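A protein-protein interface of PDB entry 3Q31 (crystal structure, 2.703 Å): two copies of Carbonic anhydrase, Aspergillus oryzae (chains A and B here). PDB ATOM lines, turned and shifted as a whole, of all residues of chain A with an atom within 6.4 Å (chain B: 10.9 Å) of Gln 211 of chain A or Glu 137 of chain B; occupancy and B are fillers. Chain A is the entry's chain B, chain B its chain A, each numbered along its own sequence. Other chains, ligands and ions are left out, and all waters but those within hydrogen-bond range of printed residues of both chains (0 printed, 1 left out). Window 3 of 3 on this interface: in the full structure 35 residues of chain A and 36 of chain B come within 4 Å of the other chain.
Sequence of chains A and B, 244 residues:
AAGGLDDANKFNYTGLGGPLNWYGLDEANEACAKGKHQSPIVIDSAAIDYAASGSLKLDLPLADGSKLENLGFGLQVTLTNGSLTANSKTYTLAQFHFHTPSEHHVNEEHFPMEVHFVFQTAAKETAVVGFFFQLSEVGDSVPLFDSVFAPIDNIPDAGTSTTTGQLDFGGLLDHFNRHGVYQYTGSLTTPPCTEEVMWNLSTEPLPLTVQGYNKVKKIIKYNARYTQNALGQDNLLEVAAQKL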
ATOM      1  N   LEU A 135      -0.512  14.676  17.037  1.00  0.00           N
ATOM      2  CA  LEU A 135      -0.096  13.305  17.299  1.00  0.00           C
ATOM      3  C   LEU A 135       1.019  13.271  18.318  1.00  0.00           C
ATOM      4  O   LEU A 135       2.016  13.988  18.173  1.00  0.00           O
ATOM      5  CB  LEU A 135       0.384  12.621  16.031  1.00  0.00           C
ATOM      6  CG  LEU A 135      -0.663  11.829  15.264  1.00  0.00           C
ATOM      7  CD1 LEU A 135      -1.447  10.982  16.232  1.00  0.00           C
ATOM      8  CD2 LEU A 135      -1.567  12.801  14.573  1.00  0.00           C
ATOM      9  N   THR A 209      -3.370   9.920  19.780  1.00  0.00           N
ATOM     10  CA  THR A 209      -2.652   8.680  19.505  1.00  0.00           C
ATOM     11  C   THR A 209      -2.980   8.191  18.111  1.00  0.00           C
ATOM     12  O   THR A 209      -4.079   8.438  17.601  1.00  0.00           O
ATOM     13  CB  THR A 209      -3.016   7.558  20.498  1.00  0.00           C
ATOM     14  OG1 THR A 209      -4.437   7.344  20.477  1.00  0.00           O
ATOM     15  CG2 THR A 209      -2.544   7.908  21.916  1.00  0.00           C
ATOM     16  N   VAL A 210      -2.028   7.497  17.492  1.00  0.00           N
ATOM     17  CA  VAL A 210      -2.248   6.972  16.149  1.00  0.00           C
ATOM     18  C   VAL A 210      -3.534   6.150  16.147  1.00  0.00           C
ATOM     19  O   VAL A 210      -4.390   6.316  15.274  1.00  0.00           O
ATOM     20  CB  VAL A 210      -1.039   6.123  15.653  1.00  0.00           C
ATOM     21  CG1 VAL A 210      -1.371   5.383  14.345  1.00  0.00           C
ATOM     22  CG2 VAL A 210       0.223   6.998  15.481  1.00  0.00           C
ATOM     23  N   GLN A 211      -3.680   5.288  17.151  1.00  0.00           N
ATOM     24  CA  GLN A 211      -4.830   4.397  17.193  1.00  0.00           C
ATOM     25  C   GLN A 211      -6.125   5.184  17.085  1.00  0.00           C
ATOM     26  O   GLN A 211      -6.989   4.878  16.240  1.00  0.00           O
ATOM     27  CB  GLN A 211      -4.826   3.540  18.457  1.00  0.00           C
ATOM     28  CG  GLN A 211      -5.910   2.475  18.422  1.00  0.00           C
ATOM     29  CD  GLN A 211      -6.487   2.177  19.784  1.00  0.00           C
ATOM     30  OE1 GLN A 211      -5.787   1.669  20.664  1.00  0.00           O
ATOM     31  NE2 GLN A 211      -7.773   2.488  19.969  1.00  0.00           N
ATOM     32  N   GLY A 212      -6.234   6.206  17.936  1.00  0.00           N
ATOM     33  CA  GLY A 212      -7.385   7.090  17.965  1.00  0.00           C
ATOM     34  C   GLY A 212      -7.618   7.843  16.674  1.00  0.00           C
ATOM     35  O   GLY A 212      -8.731   7.829  16.153  1.00  0.00           O
ATOM     36  N   TYR A 213      -6.565   8.496  16.167  1.00  0.00           N
ATOM     37  CA  TYR A 213      -6.590   9.240  14.897  1.00  0.00           C
ATOM     38  C   TYR A 213      -7.136   8.404  13.737  1.00  0.00           C
ATOM     39  O   TYR A 213      -8.012   8.849  12.974  1.00  0.00           O
ATOM     40  CB  TYR A 213      -5.185   9.755  14.538  1.00  0.00           C
ATOM     41  CG  TYR A 213      -5.061  10.431  13.165  1.00  0.00           C
ATOM     42  CD1 TYR A 213      -5.578  11.702  12.945  1.00  0.00           C
ATOM     43  CD2 TYR A 213      -4.395   9.810  12.101  1.00  0.00           C
ATOM     44  CE1 TYR A 213      -5.460  12.338  11.720  1.00  0.00           C
ATOM     45  CE2 TYR A 213      -4.267  10.442  10.852  1.00  0.00           C
ATOM     46  CZ  TYR A 213      -4.806  11.715  10.672  1.00  0.00           C
ATOM     47  OH  TYR A 213      -4.716  12.391   9.454  1.00  0.00           O
ATOM     48  N   ASN A 214      -6.608   7.196  13.593  1.00  0.00           N
ATOM     49  CA  ASN A 214      -7.045   6.346  12.500  1.00  0.00           C
ATOM     50  C   ASN A 214      -8.485   5.905  12.692  1.00  0.00           C
ATOM     51  O   ASN A 214      -9.284   5.979  11.751  1.00  0.00           O
ATOM     52  CB  ASN A 214      -6.104   5.162  12.339  1.00  0.00           C
ATOM     53  CG  ASN A 214      -4.766   5.577  11.785  1.00  0.00           C
ATOM     54  OD1 ASN A 214      -4.692   6.462  10.929  1.00  0.00           O
ATOM     55  ND2 ASN A 214      -3.693   4.954  12.267  1.00  0.00           N
ATOM     56  N   LYS A 215      -8.811   5.471  13.913  1.00  0.00           N
ATOM     57  CA  LYS A 215     -10.181   5.096  14.271  1.00  0.00           C
ATOM     58  C   LYS A 215     -11.177   6.170  13.809  1.00  0.00           C
ATOM     59  O   LYS A 215     -12.181   5.874  13.135  1.00  0.00           O
ATOM     60  CB  LYS A 215     -10.302   4.884  15.795  1.00  0.00           C
ATOM     61  CG  LYS A 215     -10.831   3.507  16.241  1.00  0.00           C
ATOM     62  CD  LYS A 215     -10.872   3.396  17.791  1.00  0.00           C
ATOM     63  CE  LYS A 215     -11.547   2.113  18.289  1.00  0.00           C
ATOM     64  NZ  LYS A 215     -10.937   0.886  17.692  1.00  0.00           N
ATOM     65  N   VAL A 216     -10.883   7.417  14.175  1.00  0.00           N
ATOM     66  CA  VAL A 216     -11.790   8.522  13.915  1.00  0.00           C
ATOM     67  C   VAL A 216     -11.806   8.829  12.429  1.00  0.00           C
ATOM     68  O   VAL A 216     -12.887   8.923  11.818  1.00  0.00           O
ATOM     69  CB  VAL A 216     -11.409   9.799  14.722  1.00  0.00           C
ATOM     70  CG1 VAL A 216     -12.311  10.964  14.346  1.00  0.00           C
ATOM     71  CG2 VAL A 216     -11.482   9.539  16.216  1.00  0.00           C
ATOM     72  N   GLU B 109     -12.081   9.175   2.178  1.00  0.00           N
ATOM     73  CA  GLU B 109     -11.148   9.251   3.302  1.00  0.00           C
ATOM     74  C   GLU B 109      -9.803   9.863   2.901  1.00  0.00           C
ATOM     75  O   GLU B 109      -9.174   9.435   1.941  1.00  0.00           O
ATOM     76  CB  GLU B 109     -10.927   7.882   3.937  1.00  0.00           C
ATOM     77  CG  GLU B 109     -10.063   7.981   5.182  1.00  0.00           C
ATOM     78  CD  GLU B 109      -9.787   6.624   5.832  1.00  0.00           C
ATOM     79  OE1 GLU B 109      -8.979   6.584   6.800  1.00  0.00           O
ATOM     80  OE2 GLU B 109     -10.378   5.605   5.386  1.00  0.00           O
ATOM     81  N   PRO B 112      -2.787  11.372   5.987  1.00  0.00           N
ATOM     82  CA  PRO B 112      -1.923  12.396   6.560  1.00  0.00           C
ATOM     83  C   PRO B 112      -0.898  12.879   5.538  1.00  0.00           C
ATOM     84  O   PRO B 112      -0.494  14.036   5.619  1.00  0.00           O
ATOM     85  CB  PRO B 112      -1.244  11.673   7.725  1.00  0.00           C
ATOM     86  CG  PRO B 112      -1.332  10.232   7.360  1.00  0.00           C
ATOM     87  CD  PRO B 112      -2.604  10.062   6.614  1.00  0.00           C
ATOM     88  N   PHE B 133       0.187   7.821   2.425  1.00  0.00           N
ATOM     89  CA  PHE B 133       0.764   7.422   3.705  1.00  0.00           C
ATOM     90  C   PHE B 133      -0.314   7.217   4.754  1.00  0.00           C
ATOM     91  O   PHE B 133      -1.306   7.947   4.779  1.00  0.00           O
ATOM     92  CB  PHE B 133       1.745   8.482   4.184  1.00  0.00           C
ATOM     93  CG  PHE B 133       3.043   8.481   3.432  1.00  0.00           C
ATOM     94  CD1 PHE B 133       4.043   7.582   3.765  1.00  0.00           C
ATOM     95  CD2 PHE B 133       3.257   9.370   2.400  1.00  0.00           C
ATOM     96  CE1 PHE B 133       5.232   7.571   3.094  1.00  0.00           C
ATOM     97  CE2 PHE B 133       4.447   9.374   1.713  1.00  0.00           C
ATOM     98  CZ  PHE B 133       5.445   8.467   2.051  1.00  0.00           C
ATOM     99  N   GLN B 134      -0.129   6.231   5.621  1.00  0.00           N
ATOM    100  CA  GLN B 134      -1.038   6.046   6.766  1.00  0.00           C
ATOM    101  C   GLN B 134      -0.250   5.829   8.055  1.00  0.00           C
ATOM    102  O   GLN B 134       0.639   4.973   8.090  1.00  0.00           O
ATOM    103  CB  GLN B 134      -1.982   4.865   6.552  1.00  0.00           C
ATOM    104  CG  GLN B 134      -2.912   4.633   7.732  1.00  0.00           C
ATOM    105  CD  GLN B 134      -4.070   5.631   7.764  1.00  0.00           C
ATOM    106  OE1 GLN B 134      -5.204   5.264   7.453  1.00  0.00           O
ATOM    107  NE2 GLN B 134      -3.788   6.901   8.137  1.00  0.00           N
ATOM    108  N   LEU B 135      -0.555   6.592   9.106  1.00  0.00           N
ATOM    109  CA  LEU B 135       0.186   6.456  10.361  1.00  0.00           C
ATOM    110  C   LEU B 135       0.214   5.006  10.837  1.00  0.00           C
ATOM    111  O   LEU B 135      -0.828   4.347  10.924  1.00  0.00           O
ATOM    112  CB  LEU B 135      -0.432   7.311  11.461  1.00  0.00           C
ATOM    113  CG  LEU B 135       0.150   8.706  11.580  1.00  0.00           C
ATOM    114  CD1 LEU B 135       1.656   8.601  11.476  1.00  0.00           C
ATOM    115  CD2 LEU B 135      -0.384   9.544  10.456  1.00  0.00           C
ATOM    116  N   SER B 136       1.409   4.512  11.145  1.00  0.00           N
ATOM    117  CA  SER B 136       1.556   3.133  11.609  1.00  0.00           C
ATOM    118  C   SER B 136       1.384   3.078  13.106  1.00  0.00           C
ATOM    119  O   SER B 136       2.087   3.783  13.849  1.00  0.00           O
ATOM    120  CB  SER B 136       2.928   2.533  11.225  1.00  0.00           C
ATOM    121  OG  SER B 136       3.010   1.144  11.562  1.00  0.00           O
ATOM    122  N   GLU B 137       0.451   2.235  13.538  1.00  0.00           N
ATOM    123  CA  GLU B 137       0.226   1.998  14.960  1.00  0.00           C
ATOM    124  C   GLU B 137       1.500   1.541  15.660  1.00  0.00           C
ATOM    125  O   GLU B 137       1.814   1.990  16.763  1.00  0.00           O
ATOM    126  CB  GLU B 137      -0.814   0.907  15.121  1.00  0.00           C
ATOM    127  CG  GLU B 137      -1.512   0.906  16.457  1.00  0.00           C
ATOM    128  CD  GLU B 137      -3.025   0.838  16.288  1.00  0.00           C
ATOM    129  OE1 GLU B 137      -3.723   0.458  17.262  1.00  0.00           O
ATOM    130  OE2 GLU B 137      -3.506   1.160  15.166  1.00  0.00           O
ATOM    131  N   VAL B 138       2.234   0.650  14.995  1.00  0.00           N
ATOM    132  CA  VAL B 138       3.363  -0.060  15.598  1.00  0.00           C
ATOM    133  C   VAL B 138       4.738   0.580  15.368  1.00  0.00           C
ATOM    134  O   VAL B 138       5.773  -0.033  15.665  1.00  0.00           O
ATOM    135  CB  VAL B 138       3.419  -1.486  15.058  1.00  0.00           C
ATOM    136  CG1 VAL B 138       2.214  -2.272  15.551  1.00  0.00           C
ATOM    137  CG2 VAL B 138       3.462  -1.462  13.530  1.00  0.00           C
ATOM    138  N   GLY B 139       4.751   1.796  14.827  1.00  0.00           N
ATOM    139  CA  GLY B 139       5.984   2.540  14.638  1.00  0.00           C
ATOM    140  C   GLY B 139       6.737   2.237  13.352  1.00  0.00           C
ATOM    141  O   GLY B 139       7.886   2.659  13.183  1.00  0.00           O
ATOM    142  N   ASP B 140       6.083   1.522  12.439  1.00  0.00           N
ATOM    143  CA  ASP B 140       6.718   1.073  11.202  1.00  0.00           C
ATOM    144  C   ASP B 140       7.024   2.194  10.224  1.00  0.00           C
ATOM    145  O   ASP B 140       6.318   3.192  10.176  1.00  0.00           O
ATOM    146  CB  ASP B 140       5.832   0.053  10.508  1.00  0.00           C
ATOM    147  CG  ASP B 140       6.502  -1.283  10.377  1.00  0.00           C
ATOM    148  OD1 ASP B 140       6.059  -2.213  11.093  1.00  0.00           O
ATOM    149  OD2 ASP B 140       7.478  -1.390   9.581  1.00  0.00           O
ATOM    150  N   SER B 141       8.056   2.018   9.413  1.00  0.00           N
ATOM    151  CA  SER B 141       8.462   3.095   8.523  1.00  0.00           C
ATOM    152  C   SER B 141       8.942   2.583   7.189  1.00  0.00           C
ATOM    153  O   SER B 141       9.207   1.387   7.028  1.00  0.00           O
ATOM    154  CB  SER B 141       9.576   3.923   9.170  1.00  0.00           C
ATOM    155  OG  SER B 141       9.522   5.262   8.707  1.00  0.00           O
ATOM    156  N   PRO B 205      -1.464   2.142   1.108  1.00  0.00           N
ATOM    157  CA  PRO B 205      -0.702   3.205   1.765  1.00  0.00           C
ATOM    158  C   PRO B 205       0.586   2.710   2.392  1.00  0.00           C
ATOM    159  O   PRO B 205       0.665   1.575   2.873  1.00  0.00           O
ATOM    160  CB  PRO B 205      -1.652   3.692   2.859  1.00  0.00           C
ATOM    161  CG  PRO B 205      -2.990   3.222   2.446  1.00  0.00           C
ATOM    162  CD  PRO B 205      -2.786   1.951   1.719  1.00  0.00           C
ATOM    163  N   LEU B 206       1.589   3.580   2.384  1.00  0.00           N
ATOM    164  CA  LEU B 206       2.837   3.308   3.057  1.00  0.00           C
ATOM    165  C   LEU B 206       2.734   3.662   4.550  1.00  0.00           C
ATOM    166  O   LEU B 206       1.979   4.566   4.930  1.00  0.00           O
ATOM    167  CB  LEU B 206       3.928   4.127   2.396  1.00  0.00           C
ATOM    168  CG  LEU B 206       4.038   3.903   0.888  1.00  0.00           C
ATOM    169  CD1 LEU B 206       5.008   4.930   0.241  1.00  0.00           C
ATOM    170  CD2 LEU B 206       4.449   2.457   0.610  1.00  0.00           C
ATOM    171  N   PRO B 207       3.498   2.943   5.393  1.00  0.00           N
ATOM    172  CA  PRO B 207       3.688   3.223   6.820  1.00  0.00           C
ATOM    173  C   PRO B 207       4.299   4.586   7.032  1.00  0.00           C
ATOM    174  O   PRO B 207       5.244   4.958   6.325  1.00  0.00           O
ATOM    175  CB  PRO B 207       4.736   2.183   7.250  1.00  0.00           C
ATOM    176  CG  PRO B 207       4.650   1.108   6.246  1.00  0.00           C
ATOM    177  CD  PRO B 207       4.264   1.762   4.957  1.00  0.00           C
ATOM    178  N   LEU B 208       3.788   5.312   8.017  1.00  0.00           N
ATOM    179  CA  LEU B 208       4.363   6.590   8.404  1.00  0.00           C
ATOM    180  C   LEU B 208       4.431   6.620   9.914  1.00  0.00           C
ATOM    181  O   LEU B 208       3.563   6.050  10.576  1.00  0.00           O
ATOM    182  CB  LEU B 208       3.498   7.739   7.885  1.00  0.00           C
ATOM    183  CG  LEU B 208       4.083   9.123   8.140  1.00  0.00           C
ATOM    184  CD1 LEU B 208       5.500   9.222   7.537  1.00  0.00           C
ATOM    185  CD2 LEU B 208       3.178  10.220   7.606  1.00  0.00           C
ATOM    186  N   THR B 209       5.455   7.260  10.465  1.00  0.00           N
ATOM    187  CA  THR B 209       5.587   7.354  11.919  1.00  0.00           C
ATOM    188  C   THR B 209       5.232   8.739  12.400  1.00  0.00           C
ATOM    189  O   THR B 209       5.439   9.728  11.675  1.00  0.00           O
ATOM    190  CB  THR B 209       7.019   7.086  12.383  1.00  0.00           C
ATOM    191  OG1 THR B 209       7.904   8.008  11.731  1.00  0.00           O
ATOM    192  CG2 THR B 209       7.416   5.659  12.069  1.00  0.00           C
ATOM    193  N   VAL B 210       4.717   8.812  13.624  1.00  0.00           N
ATOM    194  CA  VAL B 210       4.387  10.098  14.229  1.00  0.00           C
ATOM    195  C   VAL B 210       5.587  11.051  14.110  1.00  0.00           C
ATOM    196  O   VAL B 210       5.450  12.214  13.693  1.00  0.00           O
ATOM    197  CB  VAL B 210       3.943   9.950  15.729  1.00  0.00           C
ATOM    198  CG1 VAL B 210       3.803  11.309  16.405  1.00  0.00           C
ATOM    199  CG2 VAL B 210       2.639   9.177  15.835  1.00  0.00           C
ATOM    200  N   GLN B 211       6.769  10.559  14.459  1.00  0.00           N
ATOM    201  CA  GLN B 211       7.929  11.440  14.466  1.00  0.00           C
ATOM    202  C   GLN B 211       8.124  12.094  13.113  1.00  0.00           C
ATOM    203  O   GLN B 211       8.334  13.302  13.011  1.00  0.00           O
ATOM    204  CB  GLN B 211       9.194  10.686  14.840  1.00  0.00           C
ATOM    205  CG  GLN B 211      10.375  11.612  15.007  1.00  0.00           C
ATOM    206  CD  GLN B 211      11.680  10.964  14.631  1.00  0.00           C
ATOM    207  OE1 GLN B 211      12.122  10.014  15.278  1.00  0.00           O
ATOM    208  NE2 GLN B 211      12.314  11.477  13.576  1.00  0.00           N
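Glu 137 of chain B touches two residues of chain A. No residue of chain B comes within 4 Å of Thr 209 of chain A. Val 210 of chain A touches just these residues of chain B: Leu 135, Ser 136, Glu 137 and Val 210. No residue of chain B comes within 4 Å of Gly 212 of chain A. Asn 214 of chain A touches just these residues of chain B: Gln 134 (3.0 Å) and Leu 135 (3.2 Å). No residue of chain B comes within 4 Å of Lys 215 of chain A. Of the printed residues of chain B, Leu 135 of chain A touches Val 210. Printed residues of chain A within 4 Å of Pro 112 of chain B: Tyr 213. Printed residues of chain A within 4 Å of Ser 136 of chain B: Val 210.
NE2 of Gln 134 of chain B sits at hydrogen-bond distance from OD1 of Asn 214 of chain A (3.0 Å). The backbone carbonyl oxygen of Leu 135 of chain B lies within hydrogen-bond range of the side-chain amide nitrogen of Asn 214 of chain A (3.2 Å).
Leu 135 of chain A touches Val 210 of chain B, and with the chains exchanged Val 210 of chain A touches Leu 135 of chain B. Val 210 of chain A touches its own counterpart, Val 210 of chain B. 4 positions are printed for both chains.
Of the 18 printed residues of chain B, 6 touch a printed residue of chain A. Of the 9 printed residues of chain A, 5 touch a printed residue of chain B. Along chain A the printed residues that touch a printed residue of chain B span positions 135 to 214. Among the printed residues, 9 pairs touch across the chains.
The backbone carbonyl oxygen (O) of Leu 208 of chain B sits at hydrogen-bond distance from the backbone NH (N) of Ser 136 of chain B (2.7 Å). ND2 of Asn 214 of chain A lies close to O of Val 210 of chain A (3.4 Å). N of Gln 134 of chain B is in hydrogen-bond range of O of Leu 206 of chain B. The backbone NH of Leu 208 of chain B is in hydrogen-bond range of the backbone carbonyl oxygen of Gln 134 of chain B, 3.2 Å away. The backbone NH (N) of Asp 140 of chain B sits close to the side-chain hydroxyl (OG) of Ser 136 of chain B (3.2 Å).
Val 210 of chain B touches Leu 135 of chain A (CG1 to O, 3.7 Å). Val 210 of chain A touches Leu 135 of chain B (CG1 to CB, 3.6 Å). CG1 of Val 210 of chain A touches C of Ser 136 of chain B, 3.8 Å away. Val 210 of chain A touches Glu 137 of chain B (CG1 to N, 3.7 Å). CG2 of Val 210 of chain B touches CG2 of Val 210 of chain A (3.3 Å). Glu 137 of chain B touches Gln 211 of chain A. CB of Pro 112 of chain B touches OH of Tyr 213 of chain A, at 3.9 Å.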
